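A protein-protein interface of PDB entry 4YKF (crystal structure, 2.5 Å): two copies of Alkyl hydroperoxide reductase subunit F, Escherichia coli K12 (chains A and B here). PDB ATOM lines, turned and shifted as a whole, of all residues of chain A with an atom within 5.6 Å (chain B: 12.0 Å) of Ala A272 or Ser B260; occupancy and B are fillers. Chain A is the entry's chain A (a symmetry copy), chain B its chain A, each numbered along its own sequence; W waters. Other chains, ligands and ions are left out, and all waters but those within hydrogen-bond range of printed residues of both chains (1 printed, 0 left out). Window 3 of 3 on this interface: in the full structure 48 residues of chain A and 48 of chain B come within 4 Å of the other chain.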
ATOM      1  N   ILE A 229      29.708 -13.189 -29.764  1.00  0.00           N
ATOM      2  CA  ILE A 229      29.394 -11.986 -29.069  1.00  0.00           C
ATOM      3  C   ILE A 229      30.623 -11.534 -28.293  1.00  0.00           C
ATOM      4  O   ILE A 229      31.011 -10.333 -28.335  1.00  0.00           O
ATOM      5  CB  ILE A 229      28.193 -12.214 -28.148  1.00  0.00           C
ATOM      6  CG1 ILE A 229      26.965 -12.503 -29.023  1.00  0.00           C
ATOM      7  CG2 ILE A 229      28.013 -11.003 -27.279  1.00  0.00           C
ATOM      8  CD1 ILE A 229      25.683 -12.734 -28.274  1.00  0.00           C
ATOM      9  N   TYR A 258      17.131 -21.788 -18.751  1.00  0.00           N
ATOM     10  CA  TYR A 258      17.999 -20.735 -19.176  1.00  0.00           C
ATOM     11  C   TYR A 258      17.906 -19.682 -18.074  1.00  0.00           C
ATOM     12  O   TYR A 258      16.974 -18.869 -18.039  1.00  0.00           O
ATOM     13  CB  TYR A 258      17.647 -20.203 -20.576  1.00  0.00           C
ATOM     14  CG  TYR A 258      18.800 -19.450 -21.119  1.00  0.00           C
ATOM     15  CD1 TYR A 258      19.875 -20.113 -21.628  1.00  0.00           C
ATOM     16  CD2 TYR A 258      18.889 -18.054 -20.963  1.00  0.00           C
ATOM     17  CE1 TYR A 258      20.996 -19.431 -22.053  1.00  0.00           C
ATOM     18  CE2 TYR A 258      20.004 -17.338 -21.382  1.00  0.00           C
ATOM     19  CZ  TYR A 258      21.069 -18.029 -21.926  1.00  0.00           C
ATOM     20  OH  TYR A 258      22.199 -17.360 -22.345  1.00  0.00           O
ATOM     21  N   GLN A 267      12.532 -21.367 -30.409  1.00  0.00           N
ATOM     22  CA  GLN A 267      12.548 -20.504 -31.549  1.00  0.00           C
ATOM     23  C   GLN A 267      12.803 -19.103 -31.129  1.00  0.00           C
ATOM     24  O   GLN A 267      13.536 -18.404 -31.797  1.00  0.00           O
ATOM     25  CB  GLN A 267      11.241 -20.616 -32.339  1.00  0.00           C
ATOM     26  CG  GLN A 267      11.261 -21.869 -33.194  1.00  0.00           C
ATOM     27  CD  GLN A 267       9.889 -22.415 -33.497  1.00  0.00           C
ATOM     28  OE1 GLN A 267       9.443 -22.462 -34.687  1.00  0.00           O
ATOM     29  NE2 GLN A 267       9.215 -22.863 -32.448  1.00  0.00           N
ATOM     30  N   LYS A 268      12.190 -18.704 -30.034  1.00  0.00           N
ATOM     31  CA  LYS A 268      12.326 -17.370 -29.481  1.00  0.00           C
ATOM     32  C   LYS A 268      13.771 -17.155 -29.061  1.00  0.00           C
ATOM     33  O   LYS A 268      14.360 -16.096 -29.306  1.00  0.00           O
ATOM     34  CB  LYS A 268      11.416 -17.223 -28.259  1.00  0.00           C
ATOM     35  CG  LYS A 268      11.146 -15.792 -27.786  1.00  0.00           C
ATOM     36  CD  LYS A 268      10.496 -15.765 -26.379  1.00  0.00           C
ATOM     37  CE  LYS A 268      10.512 -14.410 -25.681  1.00  0.00           C
ATOM     38  NZ  LYS A 268      10.288 -13.335 -26.682  1.00  0.00           N
ATOM     39  N   LEU A 269      14.360 -18.180 -28.460  1.00  0.00           N
ATOM     40  CA  LEU A 269      15.697 -18.036 -27.912  1.00  0.00           C
ATOM     41  C   LEU A 269      16.724 -17.960 -29.066  1.00  0.00           C
ATOM     42  O   LEU A 269      17.659 -17.106 -29.066  1.00  0.00           O
ATOM     43  CB  LEU A 269      15.979 -19.172 -26.963  1.00  0.00           C
ATOM     44  CG  LEU A 269      17.348 -19.191 -26.272  1.00  0.00           C
ATOM     45  CD1 LEU A 269      17.629 -17.925 -25.458  1.00  0.00           C
ATOM     46  CD2 LEU A 269      17.370 -20.419 -25.380  1.00  0.00           C
ATOM     47  N   ALA A 270      16.518 -18.787 -30.084  1.00  0.00           N
ATOM     48  CA  ALA A 270      17.431 -18.742 -31.228  1.00  0.00           C
ATOM     49  C   ALA A 270      17.365 -17.405 -31.856  1.00  0.00           C
ATOM     50  O   ALA A 270      18.348 -16.909 -32.255  1.00  0.00           O
ATOM     51  CB  ALA A 270      17.100 -19.803 -32.273  1.00  0.00           C
ATOM     52  N   GLY A 271      16.177 -16.830 -31.939  1.00  0.00           N
ATOM     53  CA  GLY A 271      16.005 -15.510 -32.522  1.00  0.00           C
ATOM     54  C   GLY A 271      16.593 -14.407 -31.667  1.00  0.00           C
ATOM     55  O   GLY A 271      17.150 -13.443 -32.175  1.00  0.00           O
ATOM     56  N   ALA A 272      16.478 -14.574 -30.369  1.00  0.00           N
ATOM     57  CA  ALA A 272      17.074 -13.647 -29.434  1.00  0.00           C
ATOM     58  C   ALA A 272      18.618 -13.741 -29.459  1.00  0.00           C
ATOM     59  O   ALA A 272      19.306 -12.751 -29.281  1.00  0.00           O
ATOM     60  CB  ALA A 272      16.538 -13.927 -28.053  1.00  0.00           C
ATOM     61  N   LEU A 273      19.159 -14.922 -29.699  1.00  0.00           N
ATOM     62  CA  LEU A 273      20.585 -15.041 -29.962  1.00  0.00           C
ATOM     63  C   LEU A 273      21.002 -14.394 -31.249  1.00  0.00           C
ATOM     64  O   LEU A 273      22.108 -13.902 -31.379  1.00  0.00           O
ATOM     65  CB  LEU A 273      21.042 -16.505 -30.016  1.00  0.00           C
ATOM     66  CG  LEU A 273      20.977 -17.295 -28.722  1.00  0.00           C
ATOM     67  CD1 LEU A 273      21.236 -18.764 -29.030  1.00  0.00           C
ATOM     68  CD2 LEU A 273      22.013 -16.820 -27.750  1.00  0.00           C
ATOM     69  N   LYS A 274      20.163 -14.445 -32.245  1.00  0.00           N
ATOM     70  CA  LYS A 274      20.551 -13.827 -33.518  1.00  0.00           C
ATOM     71  C   LYS A 274      20.618 -12.321 -33.367  1.00  0.00           C
ATOM     72  O   LYS A 274      21.489 -11.655 -33.922  1.00  0.00           O
ATOM     73  CB  LYS A 274      19.511 -14.138 -34.578  1.00  0.00           C
ATOM     74  CG  LYS A 274      19.916 -13.691 -35.947  1.00  0.00           C
ATOM     75  CD  LYS A 274      21.228 -14.334 -36.357  1.00  0.00           C
ATOM     76  CE  LYS A 274      21.785 -13.734 -37.629  1.00  0.00           C
ATOM     77  NZ  LYS A 274      20.697 -13.556 -38.626  1.00  0.00           N
ATOM     78  N   VAL A 275      19.647 -11.800 -32.629  1.00  0.00           N
ATOM     79  CA  VAL A 275      19.577 -10.400 -32.426  1.00  0.00           C
ATOM     80  C   VAL A 275      20.784  -9.958 -31.609  1.00  0.00           C
ATOM     81  O   VAL A 275      21.315  -8.884 -31.838  1.00  0.00           O
ATOM     82  CB  VAL A 275      18.299  -9.998 -31.671  1.00  0.00           C
ATOM     83  CG1 VAL A 275      18.429  -8.573 -31.149  1.00  0.00           C
ATOM     84  CG2 VAL A 275      17.078 -10.090 -32.581  1.00  0.00           C
ATOM     85  N   HIS A 276      21.198 -10.768 -30.632  1.00  0.00           N
ATOM     86  CA  HIS A 276      22.278 -10.319 -29.770  1.00  0.00           C
ATOM     87  C   HIS A 276      23.520 -10.360 -30.596  1.00  0.00           C
ATOM     88  O   HIS A 276      24.336  -9.434 -30.530  1.00  0.00           O
ATOM     89  CB  HIS A 276      22.455 -11.156 -28.498  1.00  0.00           C
ATOM     90  CG  HIS A 276      23.221 -10.458 -27.429  1.00  0.00           C
ATOM     91  ND1 HIS A 276      23.407 -10.995 -26.179  1.00  0.00           N
ATOM     92  CD2 HIS A 276      23.811  -9.237 -27.397  1.00  0.00           C
ATOM     93  CE1 HIS A 276      24.099 -10.151 -25.429  1.00  0.00           C
ATOM     94  NE2 HIS A 276      24.357  -9.078 -26.144  1.00  0.00           N
ATOM     95  N   VAL A 277      23.624 -11.388 -31.423  1.00  0.00           N
ATOM     96  CA  VAL A 277      24.748 -11.469 -32.370  1.00  0.00           C
ATOM     97  C   VAL A 277      24.821 -10.291 -33.334  1.00  0.00           C
ATOM     98  O   VAL A 277      25.894  -9.804 -33.616  1.00  0.00           O
ATOM     99  CB  VAL A 277      24.769 -12.809 -33.157  1.00  0.00           C
ATOM    100  CG1 VAL A 277      25.889 -12.850 -34.189  1.00  0.00           C
ATOM    101  CG2 VAL A 277      24.949 -13.979 -32.205  1.00  0.00           C
ATOM    102  N   ILE B 255      24.561  -4.004 -18.544  1.00  0.00           N
ATOM    103  CA  ILE B 255      25.138  -5.295 -18.863  1.00  0.00           C
ATOM    104  C   ILE B 255      24.767  -5.681 -20.283  1.00  0.00           C
ATOM    105  O   ILE B 255      23.601  -5.843 -20.608  1.00  0.00           O
ATOM    106  CB  ILE B 255      24.609  -6.360 -17.910  1.00  0.00           C
ATOM    107  CG1 ILE B 255      25.056  -6.032 -16.494  1.00  0.00           C
ATOM    108  CG2 ILE B 255      25.080  -7.750 -18.348  1.00  0.00           C
ATOM    109  CD1 ILE B 255      24.349  -6.816 -15.387  1.00  0.00           C
ATOM    110  N   GLU B 256      25.760  -5.798 -21.139  1.00  0.00           N
ATOM    111  CA  GLU B 256      25.494  -6.065 -22.545  1.00  0.00           C
ATOM    112  C   GLU B 256      25.984  -7.436 -23.016  1.00  0.00           C
ATOM    113  O   GLU B 256      25.874  -7.733 -24.177  1.00  0.00           O
ATOM    114  CB  GLU B 256      26.089  -4.947 -23.382  1.00  0.00           C
ATOM    115  CG  GLU B 256      25.165  -3.744 -23.406  1.00  0.00           C
ATOM    116  CD  GLU B 256      25.850  -2.411 -23.586  1.00  0.00           C
ATOM    117  OE1 GLU B 256      25.164  -1.396 -23.399  1.00  0.00           O
ATOM    118  OE2 GLU B 256      27.053  -2.339 -23.913  1.00  0.00           O
ATOM    119  N   ASN B 257      26.513  -8.264 -22.107  1.00  0.00           N
ATOM    120  CA  ASN B 257      27.027  -9.583 -22.484  1.00  0.00           C
ATOM    121  C   ASN B 257      26.377 -10.770 -21.774  1.00  0.00           C
ATOM    122  O   ASN B 257      26.939 -11.829 -21.745  1.00  0.00           O
ATOM    123  CB  ASN B 257      28.544  -9.616 -22.337  1.00  0.00           C
ATOM    124  CG  ASN B 257      28.977  -9.355 -20.961  1.00  0.00           C
ATOM    125  OD1 ASN B 257      28.178  -9.278 -20.082  1.00  0.00           O
ATOM    126  ND2 ASN B 257      30.253  -9.249 -20.756  1.00  0.00           N
ATOM    127  N   TYR B 258      25.203 -10.577 -21.180  1.00  0.00           N
ATOM    128  CA  TYR B 258      24.431 -11.695 -20.736  1.00  0.00           C
ATOM    129  C   TYR B 258      23.735 -12.214 -21.993  1.00  0.00           C
ATOM    130  O   TYR B 258      22.695 -11.691 -22.414  1.00  0.00           O
ATOM    131  CB  TYR B 258      23.464 -11.334 -19.595  1.00  0.00           C
ATOM    132  CG  TYR B 258      23.027 -12.571 -18.911  1.00  0.00           C
ATOM    133  CD1 TYR B 258      23.854 -13.198 -18.029  1.00  0.00           C
ATOM    134  CD2 TYR B 258      21.835 -13.220 -19.284  1.00  0.00           C
ATOM    135  CE1 TYR B 258      23.502 -14.400 -17.454  1.00  0.00           C
ATOM    136  CE2 TYR B 258      21.451 -14.432 -18.721  1.00  0.00           C
ATOM    137  CZ  TYR B 258      22.291 -15.032 -17.803  1.00  0.00           C
ATOM    138  OH  TYR B 258      21.955 -16.238 -17.229  1.00  0.00           O
ATOM    139  N   ILE B 259      24.377 -13.232 -22.584  1.00  0.00           N
ATOM    140  CA  ILE B 259      24.029 -13.785 -23.919  1.00  0.00           C
ATOM    141  C   ILE B 259      22.514 -14.008 -24.094  1.00  0.00           C
ATOM    142  O   ILE B 259      21.886 -14.593 -23.237  1.00  0.00           O
ATOM    143  CB  ILE B 259      24.732 -15.157 -24.180  1.00  0.00           C
ATOM    144  CG1 ILE B 259      26.225 -15.077 -23.946  1.00  0.00           C
ATOM    145  CG2 ILE B 259      24.502 -15.703 -25.581  1.00  0.00           C
ATOM    146  CD1 ILE B 259      26.964 -14.064 -24.746  1.00  0.00           C
ATOM    147  N   SER B 260      22.004 -13.597 -25.239  1.00  0.00           N
ATOM    148  CA  SER B 260      20.561 -13.502 -25.611  1.00  0.00           C
ATOM    149  C   SER B 260      19.861 -12.202 -25.198  1.00  0.00           C
ATOM    150  O   SER B 260      18.859 -11.842 -25.792  1.00  0.00           O
ATOM    151  CB  SER B 260      19.708 -14.671 -25.155  1.00  0.00           C
ATOM    152  OG  SER B 260      19.279 -14.382 -23.851  1.00  0.00           O
ATOM    153  N   VAL B 261      20.414 -11.484 -24.246  1.00  0.00           N
ATOM    154  CA  VAL B 261      19.789 -10.285 -23.761  1.00  0.00           C
ATOM    155  C   VAL B 261      20.658  -9.103 -24.120  1.00  0.00           C
ATOM    156  O   VAL B 261      21.650  -8.861 -23.485  1.00  0.00           O
ATOM    157  CB  VAL B 261      19.658 -10.357 -22.242  1.00  0.00           C
ATOM    158  CG1 VAL B 261      19.052  -9.059 -21.706  1.00  0.00           C
ATOM    159  CG2 VAL B 261      18.817 -11.581 -21.856  1.00  0.00           C
ATOM    160  N   PRO B 262      20.297  -8.349 -25.146  1.00  0.00           N
ATOM    161  CA  PRO B 262      21.200  -7.282 -25.602  1.00  0.00           C
ATOM    162  C   PRO B 262      21.620  -6.249 -24.572  1.00  0.00           C
ATOM    163  O   PRO B 262      22.772  -5.786 -24.573  1.00  0.00           O
ATOM    164  CB  PRO B 262      20.385  -6.588 -26.693  1.00  0.00           C
ATOM    165  CG  PRO B 262      19.437  -7.638 -27.211  1.00  0.00           C
ATOM    166  CD  PRO B 262      19.101  -8.476 -25.996  1.00  0.00           C
ATOM    167  N   LYS B 263      20.670  -5.916 -23.702  1.00  0.00           N
ATOM    168  CA  LYS B 263      20.851  -4.880 -22.688  1.00  0.00           C
ATOM    169  C   LYS B 263      19.968  -5.095 -21.479  1.00  0.00           C
ATOM    170  O   LYS B 263      18.772  -4.986 -21.573  1.00  0.00           O
ATOM    171  CB  LYS B 263      20.561  -3.497 -23.297  1.00  0.00           C
ATOM    172  CG  LYS B 263      20.912  -2.317 -22.384  1.00  0.00           C
ATOM    173  CD  LYS B 263      20.476  -0.963 -22.965  1.00  0.00           C
ATOM    174  CE  LYS B 263      21.604   0.094 -22.828  1.00  0.00           C
ATOM    175  NZ  LYS B 263      21.156   1.529 -22.972  1.00  0.00           N
ATOM    176  N   THR B 264      20.550  -5.390 -20.323  1.00  0.00           N
ATOM    177  CA  THR B 264      19.791  -5.305 -19.070  1.00  0.00           C
ATOM    178  C   THR B 264      20.557  -4.534 -18.019  1.00  0.00           C
ATOM    179  O   THR B 264      21.487  -3.825 -18.344  1.00  0.00           O
ATOM    180  CB  THR B 264      19.305  -6.660 -18.565  1.00  0.00           C
ATOM    181  OG1 THR B 264      18.386  -6.472 -17.455  1.00  0.00           O
ATOM    182  CG2 THR B 264      20.438  -7.525 -18.157  1.00  0.00           C
ATOM    183  N   GLU B 265      20.132  -4.646 -16.770  1.00  0.00           N
ATOM    184  CA  GLU B 265      20.649  -3.838 -15.680  1.00  0.00           C
ATOM    185  C   GLU B 265      20.865  -4.737 -14.513  1.00  0.00           C
ATOM    186  O   GLU B 265      20.136  -5.695 -14.315  1.00  0.00           O
ATOM    187  CB  GLU B 265      19.660  -2.753 -15.243  1.00  0.00           C
ATOM    188  CG  GLU B 265      19.056  -1.939 -16.368  1.00  0.00           C
ATOM    189  CD  GLU B 265      20.108  -1.239 -17.221  1.00  0.00           C
ATOM    190  OE1 GLU B 265      21.072  -0.696 -16.621  1.00  0.00           O
ATOM    191  OE2 GLU B 265      19.966  -1.227 -18.485  1.00  0.00           O
ATOM    192  N   LYS B 268      17.798  -5.297 -12.319  1.00  0.00           N
ATOM    193  CA  LYS B 268      16.782  -6.034 -13.045  1.00  0.00           C
ATOM    194  C   LYS B 268      17.182  -7.500 -13.103  1.00  0.00           C
ATOM    195  O   LYS B 268      16.358  -8.399 -12.903  1.00  0.00           O
ATOM    196  CB  LYS B 268      16.664  -5.485 -14.469  1.00  0.00           C
ATOM    197  CG  LYS B 268      15.402  -5.878 -15.242  1.00  0.00           C
ATOM    198  CD  LYS B 268      15.528  -5.550 -16.752  1.00  0.00           C
ATOM    199  CE  LYS B 268      14.491  -6.213 -17.649  1.00  0.00           C
ATOM    200  NZ  LYS B 268      13.180  -6.248 -16.950  1.00  0.00           N
ATOM    201  N   LEU B 269      18.465  -7.743 -13.336  1.00  0.00           N
ATOM    202  CA  LEU B 269      18.927  -9.105 -13.532  1.00  0.00           C
ATOM    203  C   LEU B 269      18.900  -9.860 -12.182  1.00  0.00           C
ATOM    204  O   LEU B 269      18.441 -11.036 -12.088  1.00  0.00           O
ATOM    205  CB  LEU B 269      20.298  -9.089 -14.156  1.00  0.00           C
ATOM    206  CG  LEU B 269      20.955 -10.444 -14.450  1.00  0.00           C
ATOM    207  CD1 LEU B 269      20.118 -11.332 -15.373  1.00  0.00           C
ATOM    208  CD2 LEU B 269      22.308 -10.147 -15.072  1.00  0.00           C
ATOM    209  N   ALA B 272      15.413 -10.715 -11.611  1.00  0.00           N
ATOM    210  CA  ALA B 272      15.019 -11.780 -12.506  1.00  0.00           C
ATOM    211  C   ALA B 272      15.615 -13.135 -12.061  1.00  0.00           C
ATOM    212  O   ALA B 272      14.997 -14.173 -12.225  1.00  0.00           O
ATOM    213  CB  ALA B 272      15.454 -11.431 -13.907  1.00  0.00           C
ATOM    214  N   LEU B 273      16.802 -13.126 -11.482  1.00  0.00           N
ATOM    215  CA  LEU B 273      17.320 -14.323 -10.838  1.00  0.00           C
ATOM    216  C   LEU B 273      16.537 -14.723  -9.623  1.00  0.00           C
ATOM    217  O   LEU B 273      16.429 -15.891  -9.297  1.00  0.00           O
ATOM    218  CB  LEU B 273      18.783 -14.161 -10.408  1.00  0.00           C
ATOM    219  CG  LEU B 273      19.816 -14.025 -11.511  1.00  0.00           C
ATOM    220  CD1 LEU B 273      21.151 -13.638 -10.891  1.00  0.00           C
ATOM    221  CD2 LEU B 273      19.989 -15.320 -12.247  1.00  0.00           C
ATOM    222  N   HIS B 276      13.484 -16.412 -10.800  1.00  0.00           N
ATOM    223  CA  HIS B 276      13.665 -17.717 -11.415  1.00  0.00           C
ATOM    224  C   HIS B 276      13.903 -18.677 -10.298  1.00  0.00           C
ATOM    225  O   HIS B 276      13.356 -19.786 -10.312  1.00  0.00           O
ATOM    226  CB  HIS B 276      14.816 -17.778 -12.426  1.00  0.00           C
ATOM    227  CG  HIS B 276      14.721 -18.932 -13.364  1.00  0.00           C
ATOM    228  ND1 HIS B 276      15.596 -19.113 -14.405  1.00  0.00           N
ATOM    229  CD2 HIS B 276      13.822 -19.943 -13.456  1.00  0.00           C
ATOM    230  CE1 HIS B 276      15.262 -20.200 -15.086  1.00  0.00           C
ATOM    231  NE2 HIS B 276      14.190 -20.721 -14.530  1.00  0.00           N
ATOM    232  N   ILE B 497      29.491 -13.142 -15.831  1.00  0.00           N
ATOM    233  CA  ILE B 497      28.179 -13.601 -15.390  1.00  0.00           C
ATOM    234  C   ILE B 497      27.729 -14.868 -16.096  1.00  0.00           C
ATOM    235  O   ILE B 497      27.320 -15.824 -15.470  1.00  0.00           O
ATOM    236  CB  ILE B 497      27.087 -12.531 -15.493  1.00  0.00           C
ATOM    237  CG1 ILE B 497      27.503 -11.277 -14.755  1.00  0.00           C
ATOM    238  CG2 ILE B 497      25.800 -12.994 -14.813  1.00  0.00           C
ATOM    239  CD1 ILE B 497      26.713 -10.053 -15.152  1.00  0.00           C
ATOM    240  N   ILE B 498      27.859 -14.877 -17.396  1.00  0.00           N
ATOM    241  CA  ILE B 498      27.380 -16.011 -18.175  1.00  0.00           C
ATOM    242  C   ILE B 498      28.258 -17.228 -17.886  1.00  0.00           C
ATOM    243  O   ILE B 498      27.754 -18.335 -17.751  1.00  0.00           O
ATOM    244  CB  ILE B 498      27.210 -15.645 -19.662  1.00  0.00           C
ATOM    245  CG1 ILE B 498      26.361 -16.697 -20.432  1.00  0.00           C
ATOM    246  CG2 ILE B 498      28.549 -15.539 -20.313  1.00  0.00           C
ATOM    247  CD1 ILE B 498      24.861 -16.528 -20.384  1.00  0.00           C
ATOM    248  N   ILE B 499      29.547 -17.001 -17.626  1.00  0.00           N
ATOM    249  CA  ILE B 499      30.444 -18.069 -17.240  1.00  0.00           C
ATOM    250  C   ILE B 499      30.088 -18.515 -15.847  1.00  0.00           C
ATOM    251  O   ILE B 499      29.956 -19.711 -15.591  1.00  0.00           O
ATOM    252  CB  ILE B 499      31.872 -17.597 -17.308  1.00  0.00           C
ATOM    253  CG1 ILE B 499      32.216 -17.212 -18.750  1.00  0.00           C
ATOM    254  CG2 ILE B 499      32.840 -18.685 -16.830  1.00  0.00           C
ATOM    255  CD1 ILE B 499      33.450 -16.366 -18.897  1.00  0.00           C
ATOM    256  N   THR B 501      27.151 -18.405 -14.331  1.00  0.00           N
ATOM    257  CA  THR B 501      25.961 -19.245 -14.273  1.00  0.00           C
ATOM    258  C   THR B 501      26.243 -20.647 -14.803  1.00  0.00           C
ATOM    259  O   THR B 501      25.734 -21.615 -14.316  1.00  0.00           O
ATOM    260  CB  THR B 501      24.751 -18.684 -15.002  1.00  0.00           C
ATOM    261  OG1 THR B 501      25.153 -18.142 -16.257  1.00  0.00           O
ATOM    262  CG2 THR B 501      24.211 -17.622 -14.269  1.00  0.00           C
HETATM  263  O   HOH W   1      24.511  -6.236 -26.642  1.00  0.00           O
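Among the printed residues, pairs that only touch across the chains: His A276 with Val B261 (3.4 Å), Tyr A258 with Ile B498 (3.4 Å), Leu A273 with Ile B259 (3.5 Å), Ala A272 with Ser B260 (3.6 Å), His A276 with Ile B259 (3.6 Å), Tyr A258 with His B276 (3.7 Å), His A276 with Tyr B258 (3.7 Å), His A276 with Pro B262 (3.7 Å), Leu A269 with Ser B260 (3.9 Å), Tyr A258 with Ser B260 (3.9 Å) and Ile A229 with Ile B259 (3.98 Å).
O of Ile B259 sits at hydrogen-bond distance from OH of Tyr A258 (2.9 Å). N of Ser B260 is in hydrogen-bond range of ND1 of His A276. The backbone carbonyl oxygen (O) of Glu B256 is in hydrogen-bond range of a ring nitrogen (NE2) of His A276, 2.8 Å away.
Water W1 lies within hydrogen-bond range of O of Pro B262 (2.7 Å), NE2 of His A276 (2.9 Å) and O of Glu B256 (3.2 Å).
The backbone carbonyl oxygen (O) of Ile B498 is in hydrogen-bond range of the side-chain hydroxyl (OG1) of Thr B501, 3.0 Å away.
Of the 20 printed residues of chain B, 8 touch a printed residue of chain A. Of the 13 printed residues of chain A, 6 touch a printed residue of chain B.
Of the printed residues of chain A, Ser B260 touches Tyr A258, Leu A269, Ala A272 and His A276. No residue of chain B comes within 4 Å of Ala A270. Of chain B, only Ile B259 (3.5 Å) comes within 4 Å of Leu A273. No residue of chain B comes within 4 Å of Val A275. Of the printed residues of chain A, Ile B259 touches Ile A229, Tyr A258, Leu A273 and His A276. Printed residues of chain B within 4 Å of Ile A229: Ile B259. Of the printed residues of chain A, His B276 touches Tyr A258 (3.7 Å). Of the printed residues of chain A, Val B261 touches His A276 (3.4 Å). Printed residues of chain B within 4 Å of Tyr A258: Ile B259 (2.9 Å), Ser B260 (3.9 Å), His B276 (3.7 Å) and Ile B498 (3.4 Å). Leu B273 touches none of the printed residues of chain A. Ile B255 touches none of the printed residues of chain A. The nearest residue of chain B that does not touch Ala A272 is Val B261 (5.3 Å). The nearest residue of chain A that does not touch Ser B260 is Leu A273 (4.1 Å). The nearest printed residue of chain A that does not touch Ile B259 is Leu A269 (5.8 Å).
Tyr A258 touches His B276, and with the chains exchanged His A276 touches Tyr B258. Positions printed for both chains: 258, 268, 269, 272, 273 and 276.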
